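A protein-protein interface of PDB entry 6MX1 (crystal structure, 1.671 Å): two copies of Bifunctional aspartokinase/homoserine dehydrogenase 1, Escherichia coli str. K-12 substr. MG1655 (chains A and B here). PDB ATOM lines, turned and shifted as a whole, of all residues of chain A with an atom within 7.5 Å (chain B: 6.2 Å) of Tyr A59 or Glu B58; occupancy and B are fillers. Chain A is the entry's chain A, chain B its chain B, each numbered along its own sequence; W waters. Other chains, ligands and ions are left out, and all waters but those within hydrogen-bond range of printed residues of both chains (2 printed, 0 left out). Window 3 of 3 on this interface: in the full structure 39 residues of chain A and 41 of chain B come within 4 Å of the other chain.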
ATOM      1  N   VAL A  23      30.458  25.931  17.491  1.00  0.00           N
ATOM      2  CA  VAL A  23      29.605  27.099  17.503  1.00  0.00           C
ATOM      3  C   VAL A  23      28.197  26.628  17.838  1.00  0.00           C
ATOM      4  O   VAL A  23      27.695  25.689  17.214  1.00  0.00           O
ATOM      5  CB  VAL A  23      29.606  27.785  16.126  1.00  0.00           C
ATOM      6  CG1 VAL A  23      28.897  29.141  16.188  1.00  0.00           C
ATOM      7  CG2 VAL A  23      31.044  27.895  15.637  1.00  0.00           C
ATOM      8  N   SER A  24      27.602  27.204  18.877  1.00  0.00           N
ATOM      9  CA  SER A  24      26.277  26.752  19.270  1.00  0.00           C
ATOM     10  C   SER A  24      25.552  27.935  19.869  1.00  0.00           C
ATOM     11  O   SER A  24      26.142  28.984  20.138  1.00  0.00           O
ATOM     12  CB  SER A  24      26.364  25.588  20.261  1.00  0.00           C
ATOM     13  OG  SER A  24      26.947  26.032  21.445  1.00  0.00           O
ATOM     14  N   GLY A  25      24.263  27.767  20.104  1.00  0.00           N
ATOM     15  CA  GLY A  25      23.565  28.806  20.811  1.00  0.00           C
ATOM     16  C   GLY A  25      22.097  28.551  20.698  1.00  0.00           C
ATOM     17  O   GLY A  25      21.661  27.744  19.874  1.00  0.00           O
ATOM     18  N   MET A  28      20.737  29.321  17.202  1.00  0.00           N
ATOM     19  CA  MET A  28      21.365  28.759  16.012  1.00  0.00           C
ATOM     20  C   MET A  28      20.424  27.893  15.184  1.00  0.00           C
ATOM     21  O   MET A  28      20.598  27.771  13.963  1.00  0.00           O
ATOM     22  CB  MET A  28      22.600  27.965  16.408  1.00  0.00           C
ATOM     23  CG  MET A  28      23.713  28.247  15.462  1.00  0.00           C
ATOM     24  SD  MET A  28      25.084  27.145  15.615  1.00  0.00           S
ATOM     25  CE  MET A  28      24.328  25.518  15.443  1.00  0.00           C
ATOM     26  N   LYS A  29      19.429  27.284  15.818  1.00  0.00           N
ATOM     27  CA  LYS A  29      18.422  26.556  15.062  1.00  0.00           C
ATOM     28  C   LYS A  29      17.500  27.481  14.266  1.00  0.00           C
ATOM     29  O   LYS A  29      16.810  27.028  13.341  1.00  0.00           O
ATOM     30  CB  LYS A  29      17.599  25.717  16.028  1.00  0.00           C
ATOM     31  CG  LYS A  29      16.790  24.652  15.356  1.00  0.00           C
ATOM     32  CD  LYS A  29      15.507  24.412  16.093  1.00  0.00           C
ATOM     33  CE  LYS A  29      14.600  23.553  15.252  1.00  0.00           C
ATOM     34  NZ  LYS A  29      13.866  22.580  16.092  1.00  0.00           N
ATOM     35  N   THR A  53      31.393  18.926  11.138  1.00  0.00           N
ATOM     36  CA  THR A  53      30.350  17.993  11.568  1.00  0.00           C
ATOM     37  C   THR A  53      29.259  18.764  12.286  1.00  0.00           C
ATOM     38  O   THR A  53      29.518  19.708  13.040  1.00  0.00           O
ATOM     39  CB  THR A  53      31.028  16.868  12.422  1.00  0.00           C
ATOM     40  OG1 THR A  53      30.056  15.892  12.798  1.00  0.00           O
ATOM     41  CG2 THR A  53      31.684  17.427  13.671  1.00  0.00           C
ATOM     42  N   GLN A  54      27.975  18.404  12.010  1.00  0.00           N
ATOM     43  CA  GLN A  54      26.884  18.946  12.793  1.00  0.00           C
ATOM     44  C   GLN A  54      25.835  17.849  12.884  1.00  0.00           C
ATOM     45  O   GLN A  54      25.329  17.378  11.859  1.00  0.00           O
ATOM     46  CB  GLN A  54      26.229  20.193  12.136  1.00  0.00           C
ATOM     47  CG  GLN A  54      25.156  20.750  13.031  1.00  0.00           C
ATOM     48  CD  GLN A  54      24.474  21.978  12.472  1.00  0.00           C
ATOM     49  OE1 GLN A  54      24.554  22.245  11.255  1.00  0.00           O
ATOM     50  NE2 GLN A  54      23.796  22.746  13.352  1.00  0.00           N
ATOM     51  N   SER A  55      25.539  17.400  14.126  1.00  0.00           N
ATOM     52  CA  SER A  55      24.735  16.175  14.209  1.00  0.00           C
ATOM     53  C   SER A  55      23.241  16.425  14.122  1.00  0.00           C
ATOM     54  O   SER A  55      22.483  15.480  13.891  1.00  0.00           O
ATOM     55  CB  SER A  55      25.021  15.390  15.525  1.00  0.00           C
ATOM     56  OG  SER A  55      24.593  16.108  16.662  1.00  0.00           O
ATOM     57  N   SER A  56      22.803  17.647  14.369  1.00  0.00           N
ATOM     58  CA  SER A  56      21.404  17.987  14.148  1.00  0.00           C
ATOM     59  C   SER A  56      21.341  19.495  14.253  1.00  0.00           C
ATOM     60  O   SER A  56      22.282  20.125  14.716  1.00  0.00           O
ATOM     61  CB  SER A  56      20.463  17.302  15.141  1.00  0.00           C
ATOM     62  OG  SER A  56      20.392  18.046  16.342  1.00  0.00           O
ATOM     63  N   SER A  57      20.211  20.074  13.814  1.00  0.00           N
ATOM     64  CA  SER A  57      20.077  21.531  13.762  1.00  0.00           C
ATOM     65  C   SER A  57      20.146  22.179  15.146  1.00  0.00           C
ATOM     66  O   SER A  57      20.410  23.383  15.240  1.00  0.00           O
ATOM     67  CB  SER A  57      18.744  21.904  13.110  1.00  0.00           C
ATOM     68  OG  SER A  57      17.693  21.551  13.995  1.00  0.00           O
ATOM     69  N   GLU A  58      19.928  21.407  16.214  1.00  0.00           N
ATOM     70  CA  GLU A  58      20.002  21.910  17.575  1.00  0.00           C
ATOM     71  C   GLU A  58      21.385  21.766  18.202  1.00  0.00           C
ATOM     72  O   GLU A  58      21.617  22.303  19.288  1.00  0.00           O
ATOM     73  CB  GLU A  58      18.995  21.178  18.449  1.00  0.00           C
ATOM     74  CG  GLU A  58      17.567  21.320  17.965  1.00  0.00           C
ATOM     75  CD  GLU A  58      16.574  20.900  19.017  1.00  0.00           C
ATOM     76  OE1 GLU A  58      16.580  19.700  19.361  1.00  0.00           O
ATOM     77  OE2 GLU A  58      15.771  21.746  19.479  1.00  0.00           O
ATOM     78  N   TYR A  59      22.290  21.032  17.582  1.00  0.00           N
ATOM     79  CA  TYR A  59      23.586  20.785  18.205  1.00  0.00           C
ATOM     80  C   TYR A  59      24.647  21.621  17.495  1.00  0.00           C
ATOM     81  O   TYR A  59      24.413  22.159  16.421  1.00  0.00           O
ATOM     82  CB  TYR A  59      23.938  19.284  18.167  1.00  0.00           C
ATOM     83  CG  TYR A  59      23.188  18.442  19.201  1.00  0.00           C
ATOM     84  CD1 TYR A  59      23.487  18.544  20.571  1.00  0.00           C
ATOM     85  CD2 TYR A  59      22.211  17.522  18.813  1.00  0.00           C
ATOM     86  CE1 TYR A  59      22.813  17.772  21.527  1.00  0.00           C
ATOM     87  CE2 TYR A  59      21.504  16.747  19.783  1.00  0.00           C
ATOM     88  CZ  TYR A  59      21.837  16.874  21.129  1.00  0.00           C
ATOM     89  OH  TYR A  59      21.197  16.125  22.087  1.00  0.00           O
ATOM     90  N   SER A  60      25.828  21.732  18.121  1.00  0.00           N
ATOM     91  CA  SER A  60      26.817  22.659  17.597  1.00  0.00           C
ATOM     92  C   SER A  60      27.341  22.254  16.205  1.00  0.00           C
ATOM     93  O   SER A  60      27.424  21.069  15.843  1.00  0.00           O
ATOM     94  CB  SER A  60      27.971  22.797  18.622  1.00  0.00           C
ATOM     95  OG  SER A  60      28.649  21.574  18.804  1.00  0.00           O
ATOM     96  N   ILE A  61      27.723  23.260  15.429  1.00  0.00           N
ATOM     97  CA  ILE A  61      28.579  23.007  14.264  1.00  0.00           C
ATOM     98  C   ILE A  61      29.995  22.960  14.803  1.00  0.00           C
ATOM     99  O   ILE A  61      30.424  23.933  15.442  1.00  0.00           O
ATOM    100  CB  ILE A  61      28.457  24.110  13.217  1.00  0.00           C
ATOM    101  CG1 ILE A  61      27.055  24.193  12.642  1.00  0.00           C
ATOM    102  CG2 ILE A  61      29.464  23.814  12.089  1.00  0.00           C
ATOM    103  CD1 ILE A  61      26.809  25.445  11.713  1.00  0.00           C
ATOM    104  N   SER A  62      30.710  21.855  14.549  1.00  0.00           N
ATOM    105  CA  SER A  62      32.110  21.747  14.941  1.00  0.00           C
ATOM    106  C   SER A  62      32.973  21.574  13.699  1.00  0.00           C
ATOM    107  O   SER A  62      32.529  21.007  12.695  1.00  0.00           O
ATOM    108  CB  SER A  62      32.360  20.566  15.910  1.00  0.00           C
ATOM    109  OG  SER A  62      31.622  20.821  17.098  1.00  0.00           O
ATOM    110  N   SER B  22      19.070   9.880  16.129  1.00  0.00           N
ATOM    111  CA  SER B  22      19.995  10.625  17.008  1.00  0.00           C
ATOM    112  C   SER B  22      19.918  10.013  18.392  1.00  0.00           C
ATOM    113  O   SER B  22      18.825   9.796  18.929  1.00  0.00           O
ATOM    114  CB  SER B  22      19.665  12.121  17.110  1.00  0.00           C
ATOM    115  OG  SER B  22      19.782  12.758  15.841  1.00  0.00           O
ATOM    116  N   VAL B  23      21.103   9.708  18.958  1.00  0.00           N
ATOM    117  CA  VAL B  23      21.202   9.068  20.264  1.00  0.00           C
ATOM    118  C   VAL B  23      21.825  10.092  21.195  1.00  0.00           C
ATOM    119  O   VAL B  23      22.929  10.559  20.950  1.00  0.00           O
ATOM    120  CB  VAL B  23      22.077   7.810  20.195  1.00  0.00           C
ATOM    121  CG1 VAL B  23      22.087   7.051  21.543  1.00  0.00           C
ATOM    122  CG2 VAL B  23      21.560   6.968  19.124  1.00  0.00           C
ATOM    123  N   SER B  24      21.096  10.477  22.244  1.00  0.00           N
ATOM    124  CA  SER B  24      21.546  11.570  23.097  1.00  0.00           C
ATOM    125  C   SER B  24      21.206  11.263  24.552  1.00  0.00           C
ATOM    126  O   SER B  24      20.257  10.547  24.845  1.00  0.00           O
ATOM    127  CB  SER B  24      20.910  12.904  22.732  1.00  0.00           C
ATOM    128  OG  SER B  24      20.871  13.120  21.356  1.00  0.00           O
ATOM    129  N   GLY B  25      21.955  11.854  25.460  1.00  0.00           N
ATOM    130  CA  GLY B  25      21.636  11.687  26.867  1.00  0.00           C
ATOM    131  C   GLY B  25      22.824  11.957  27.721  1.00  0.00           C
ATOM    132  O   GLY B  25      23.961  11.980  27.241  1.00  0.00           O
ATOM    133  N   PRO B  26      22.563  12.098  29.024  1.00  0.00           N
ATOM    134  CA  PRO B  26      23.626  12.341  30.014  1.00  0.00           C
ATOM    135  C   PRO B  26      24.738  11.333  29.950  1.00  0.00           C
ATOM    136  O   PRO B  26      25.930  11.683  30.117  1.00  0.00           O
ATOM    137  CB  PRO B  26      22.854  12.220  31.348  1.00  0.00           C
ATOM    138  CG  PRO B  26      21.430  12.443  31.024  1.00  0.00           C
ATOM    139  CD  PRO B  26      21.219  11.983  29.629  1.00  0.00           C
ATOM    140  N   MET B  28      26.002   9.806  27.373  1.00  0.00           N
ATOM    141  CA  MET B  28      26.871   9.839  26.189  1.00  0.00           C
ATOM    142  C   MET B  28      28.226  10.437  26.502  1.00  0.00           C
ATOM    143  O   MET B  28      29.173  10.188  25.741  1.00  0.00           O
ATOM    144  CB  MET B  28      26.248  10.636  25.018  1.00  0.00           C
ATOM    145  CG  MET B  28      24.942   9.955  24.377  1.00  0.00           C
ATOM    146  SD  MET B  28      25.196   8.227  23.802  1.00  0.00           S
ATOM    147  CE  MET B  28      25.869   8.541  22.179  1.00  0.00           C
ATOM    148  N   LYS B  29      28.328  11.255  27.526  1.00  0.00           N
ATOM    149  CA  LYS B  29      29.629  11.859  27.882  1.00  0.00           C
ATOM    150  C   LYS B  29      29.996  11.172  29.184  1.00  0.00           C
ATOM    151  O   LYS B  29      29.445  11.498  30.238  1.00  0.00           O
ATOM    152  CB  LYS B  29      29.567  13.367  28.034  1.00  0.00           C
ATOM    153  CG  LYS B  29      30.952  14.017  28.188  1.00  0.00           C
ATOM    154  CD  LYS B  29      30.843  15.498  28.499  1.00  0.00           C
ATOM    155  CE  LYS B  29      31.888  16.298  27.717  1.00  0.00           C
ATOM    156  NZ  LYS B  29      31.571  17.751  27.583  1.00  0.00           N
ATOM    157  N   SER B  55      29.054  15.962  17.016  1.00  0.00           N
ATOM    158  CA  SER B  55      29.599  17.327  16.988  1.00  0.00           C
ATOM    159  C   SER B  55      29.511  18.110  18.276  1.00  0.00           C
ATOM    160  O   SER B  55      30.207  19.128  18.410  1.00  0.00           O
ATOM    161  CB  SER B  55      28.884  18.143  15.891  1.00  0.00           C
ATOM    162  OG  SER B  55      27.495  18.318  16.229  1.00  0.00           O
ATOM    163  N   SER B  56      28.657  17.735  19.218  1.00  0.00           N
ATOM    164  CA  SER B  56      28.474  18.619  20.356  1.00  0.00           C
ATOM    165  C   SER B  56      29.280  18.154  21.567  1.00  0.00           C
ATOM    166  O   SER B  56      29.658  16.985  21.673  1.00  0.00           O
ATOM    167  CB  SER B  56      26.993  18.702  20.727  1.00  0.00           C
ATOM    168  OG  SER B  56      26.564  17.467  21.210  1.00  0.00           O
ATOM    169  N   SER B  57      29.474  19.078  22.481  1.00  0.00           N
ATOM    170  CA  SER B  57      30.128  18.749  23.743  1.00  0.00           C
ATOM    171  C   SER B  57      29.315  17.751  24.569  1.00  0.00           C
ATOM    172  O   SER B  57      29.861  17.150  25.509  1.00  0.00           O
ATOM    173  CB  SER B  57      30.390  20.016  24.544  1.00  0.00           C
ATOM    174  OG  SER B  57      29.180  20.647  24.913  1.00  0.00           O
ATOM    175  N   GLU B  58      28.033  17.546  24.248  1.00  0.00           N
ATOM    176  CA  GLU B  58      27.272  16.520  24.959  1.00  0.00           C
ATOM    177  C   GLU B  58      27.353  15.164  24.285  1.00  0.00           C
ATOM    178  O   GLU B  58      26.788  14.191  24.793  1.00  0.00           O
ATOM    179  CB  GLU B  58      25.819  16.970  25.113  1.00  0.00           C
ATOM    180  CG  GLU B  58      25.749  18.303  25.851  1.00  0.00           C
ATOM    181  CD  GLU B  58      24.354  18.871  25.897  1.00  0.00           C
ATOM    182  OE1 GLU B  58      24.119  19.823  26.686  1.00  0.00           O
ATOM    183  OE2 GLU B  58      23.500  18.358  25.139  1.00  0.00           O
ATOM    184  N   TYR B  59      28.070  15.077  23.167  1.00  0.00           N
ATOM    185  CA  TYR B  59      28.429  13.828  22.504  1.00  0.00           C
ATOM    186  C   TYR B  59      27.233  13.069  21.966  1.00  0.00           C
ATOM    187  O   TYR B  59      27.308  11.849  21.761  1.00  0.00           O
ATOM    188  CB  TYR B  59      29.237  12.902  23.416  1.00  0.00           C
ATOM    189  CG  TYR B  59      30.641  13.364  23.723  1.00  0.00           C
ATOM    190  CD1 TYR B  59      31.138  14.589  23.278  1.00  0.00           C
ATOM    191  CD2 TYR B  59      31.473  12.552  24.451  1.00  0.00           C
ATOM    192  CE1 TYR B  59      32.470  14.986  23.633  1.00  0.00           C
ATOM    193  CE2 TYR B  59      32.746  12.944  24.802  1.00  0.00           C
ATOM    194  CZ  TYR B  59      33.236  14.139  24.400  1.00  0.00           C
ATOM    195  OH  TYR B  59      34.550  14.439  24.801  1.00  0.00           O
ATOM    196  N   SER B  60      26.156  13.779  21.588  1.00  0.00           N
ATOM    197  CA  SER B  60      25.106  13.106  20.824  1.00  0.00           C
ATOM    198  C   SER B  60      25.628  12.577  19.482  1.00  0.00           C
ATOM    199  O   SER B  60      26.464  13.217  18.823  1.00  0.00           O
ATOM    200  CB  SER B  60      23.960  14.093  20.606  1.00  0.00           C
ATOM    201  OG  SER B  60      22.956  13.454  19.798  1.00  0.00           O
ATOM    202  N   SER B  62      24.522  11.176  15.630  1.00  0.00           N
ATOM    203  CA  SER B  62      23.461  11.012  14.637  1.00  0.00           C
ATOM    204  C   SER B  62      23.990  10.114  13.520  1.00  0.00           C
ATOM    205  O   SER B  62      25.186  10.171  13.185  1.00  0.00           O
ATOM    206  CB  SER B  62      22.995  12.363  14.022  1.00  0.00           C
ATOM    207  OG  SER B  62      22.259  13.196  14.921  1.00  0.00           O
ATOM    208  N   GLU B  91      18.275   9.621  26.562  1.00  0.00           N
ATOM    209  CA  GLU B  91      16.954  10.135  26.296  1.00  0.00           C
ATOM    210  C   GLU B  91      16.322   9.312  25.185  1.00  0.00           C
ATOM    211  O   GLU B  91      17.000   8.535  24.526  1.00  0.00           O
ATOM    212  CB  GLU B  91      17.062  11.592  25.859  1.00  0.00           C
ATOM    213  CG  GLU B  91      17.487  12.485  26.995  1.00  0.00           C
ATOM    214  CD  GLU B  91      18.132  13.806  26.596  1.00  0.00           C
ATOM    215  OE1 GLU B  91      18.111  14.191  25.405  1.00  0.00           O
ATOM    216  OE2 GLU B  91      18.668  14.468  27.516  1.00  0.00           O
HETATM  217  O   HOH W   1      26.630  15.751  18.490  1.00  0.00           O
HETATM  218  O   HOH W   2      22.621  14.389  17.421  1.00  0.00           O
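Of the 15 printed residues of chain B, 6 touch a printed residue of chain A. Among the printed residues, 11 pairs touch across the chains. Among the printed residues, no Asp or Glu carboxylate lies within 4 Å of a Lys or Arg side-chain nitrogen of the other chain.
OG of Ser B24 lies within hydrogen-bond range of OG of Ser B60, 2.6 Å away. O of Ser A62 lies within hydrogen-bond range of N of Thr A53 (2.8 Å). The backbone carbonyl oxygen of Tyr A59 is in hydrogen-bond range of the side-chain amide nitrogen of Gln A54, at 3.2 Å. The side-chain hydroxyl of Ser B62 lies within hydrogen-bond range of the side-chain hydroxyl of Ser B22, 2.7 Å away. N of Glu B91 is in hydrogen-bond range of O of Ser B24, at 2.8 Å. The backbone carbonyl oxygen (O) of Ser A56 lies within hydrogen-bond range of the side-chain amide nitrogen (NE2) of Gln A54, at 3.3 Å.
O of Ser A55 lies within hydrogen-bond range of OG of Ser B62 (2.5 Å). The side-chain hydroxyl of Ser B55 lies within hydrogen-bond range of the backbone carbonyl oxygen of Ser A60, 2.8 Å away. N of Ser A55 is in hydrogen-bond range of OG of Ser B55 (3.0 Å). OG of Ser A62 sits at hydrogen-bond distance from O of Ser B55 (2.6 Å). The side-chain hydroxyl of Ser B24 lies within hydrogen-bond range of the side-chain hydroxyl of Tyr A59 (3.1 Å).
Ser A55 touches Ser B62, and with the chains exchanged Ser A62 touches Ser B55. Tyr A59 touches Ser B24, but with the chains exchanged Ser A24 does not touch Tyr B59 (11.0 Å). Tyr A59 touches Glu B58, but with the chains exchanged Glu A58 does not touch Tyr B59 (10.4 Å). Ser A60 touches Ser B55, but with the chains exchanged Ser A55 does not touch Ser B60 (4.1 Å). Of the 11 pairs that touch across the chains among the printed residues, 3 have their exchanged pair printed and touching as well.
Water W1 lies within hydrogen-bond range of the backbone carbonyl oxygen (O) of Ser B60 (2.6 Å), the side-chain hydroxyl (OG) of Ser A55 (2.8 Å), the backbone NH (N) of Ser B55 (2.8 Å) and the backbone NH (N) of Ser B56 (2.9 Å). Water W2 lies within hydrogen-bond range of the side-chain hydroxyl of Ser B60, the side-chain hydroxyl of Ser A55 and the side-chain hydroxyl of Ser B62.
Of the printed residues of chain B, Tyr A59 touches Ser B24, Ser B56, Glu B58 and Ser B60. Glu B58 touches just one residue of chain A: Tyr A59. Printed residues of chain A within 4 Å of Ser B60: Tyr A59. Of the printed residues of chain B, Ser A62 touches Ser B55 (2.6 Å). Printed residues of chain A within 4 Å of Ser B55: Thr A53, Gln A54, Ser A55, Ser A60 and Ser A62. Of the printed residues of chain B, Ser A60 touches Ser B55 and Ser B56. Printed residues of chain A within 4 Å of Ser B24: Tyr A59 (3.1 Å). Tyr B59 touches none of the printed residues of chain A. Met B28 touches none of the printed residues of chain A. The nearest residue of chain A that does not touch Glu B58 is Ser A60 (6.8 Å). The nearest printed residue of chain A that does not touch Ser B24 is Ser A55 (6.7 Å).
O of Thr A53 touches CB of Ser B55 (3.3 Å). Gln A54 touches Ser B55 (CA to OG, 3.5 Å). OG of Ser B56 touches CD1 of Tyr A59, 3.3 Å away. Glu B58 touches Tyr A59 (OE2 to CE1, 3.7 Å). Ser B60 touches Tyr A59 (CB to CZ, 3.5 Å). Ser A60 touches Ser B56 (OG to CA, 3.3 Å).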
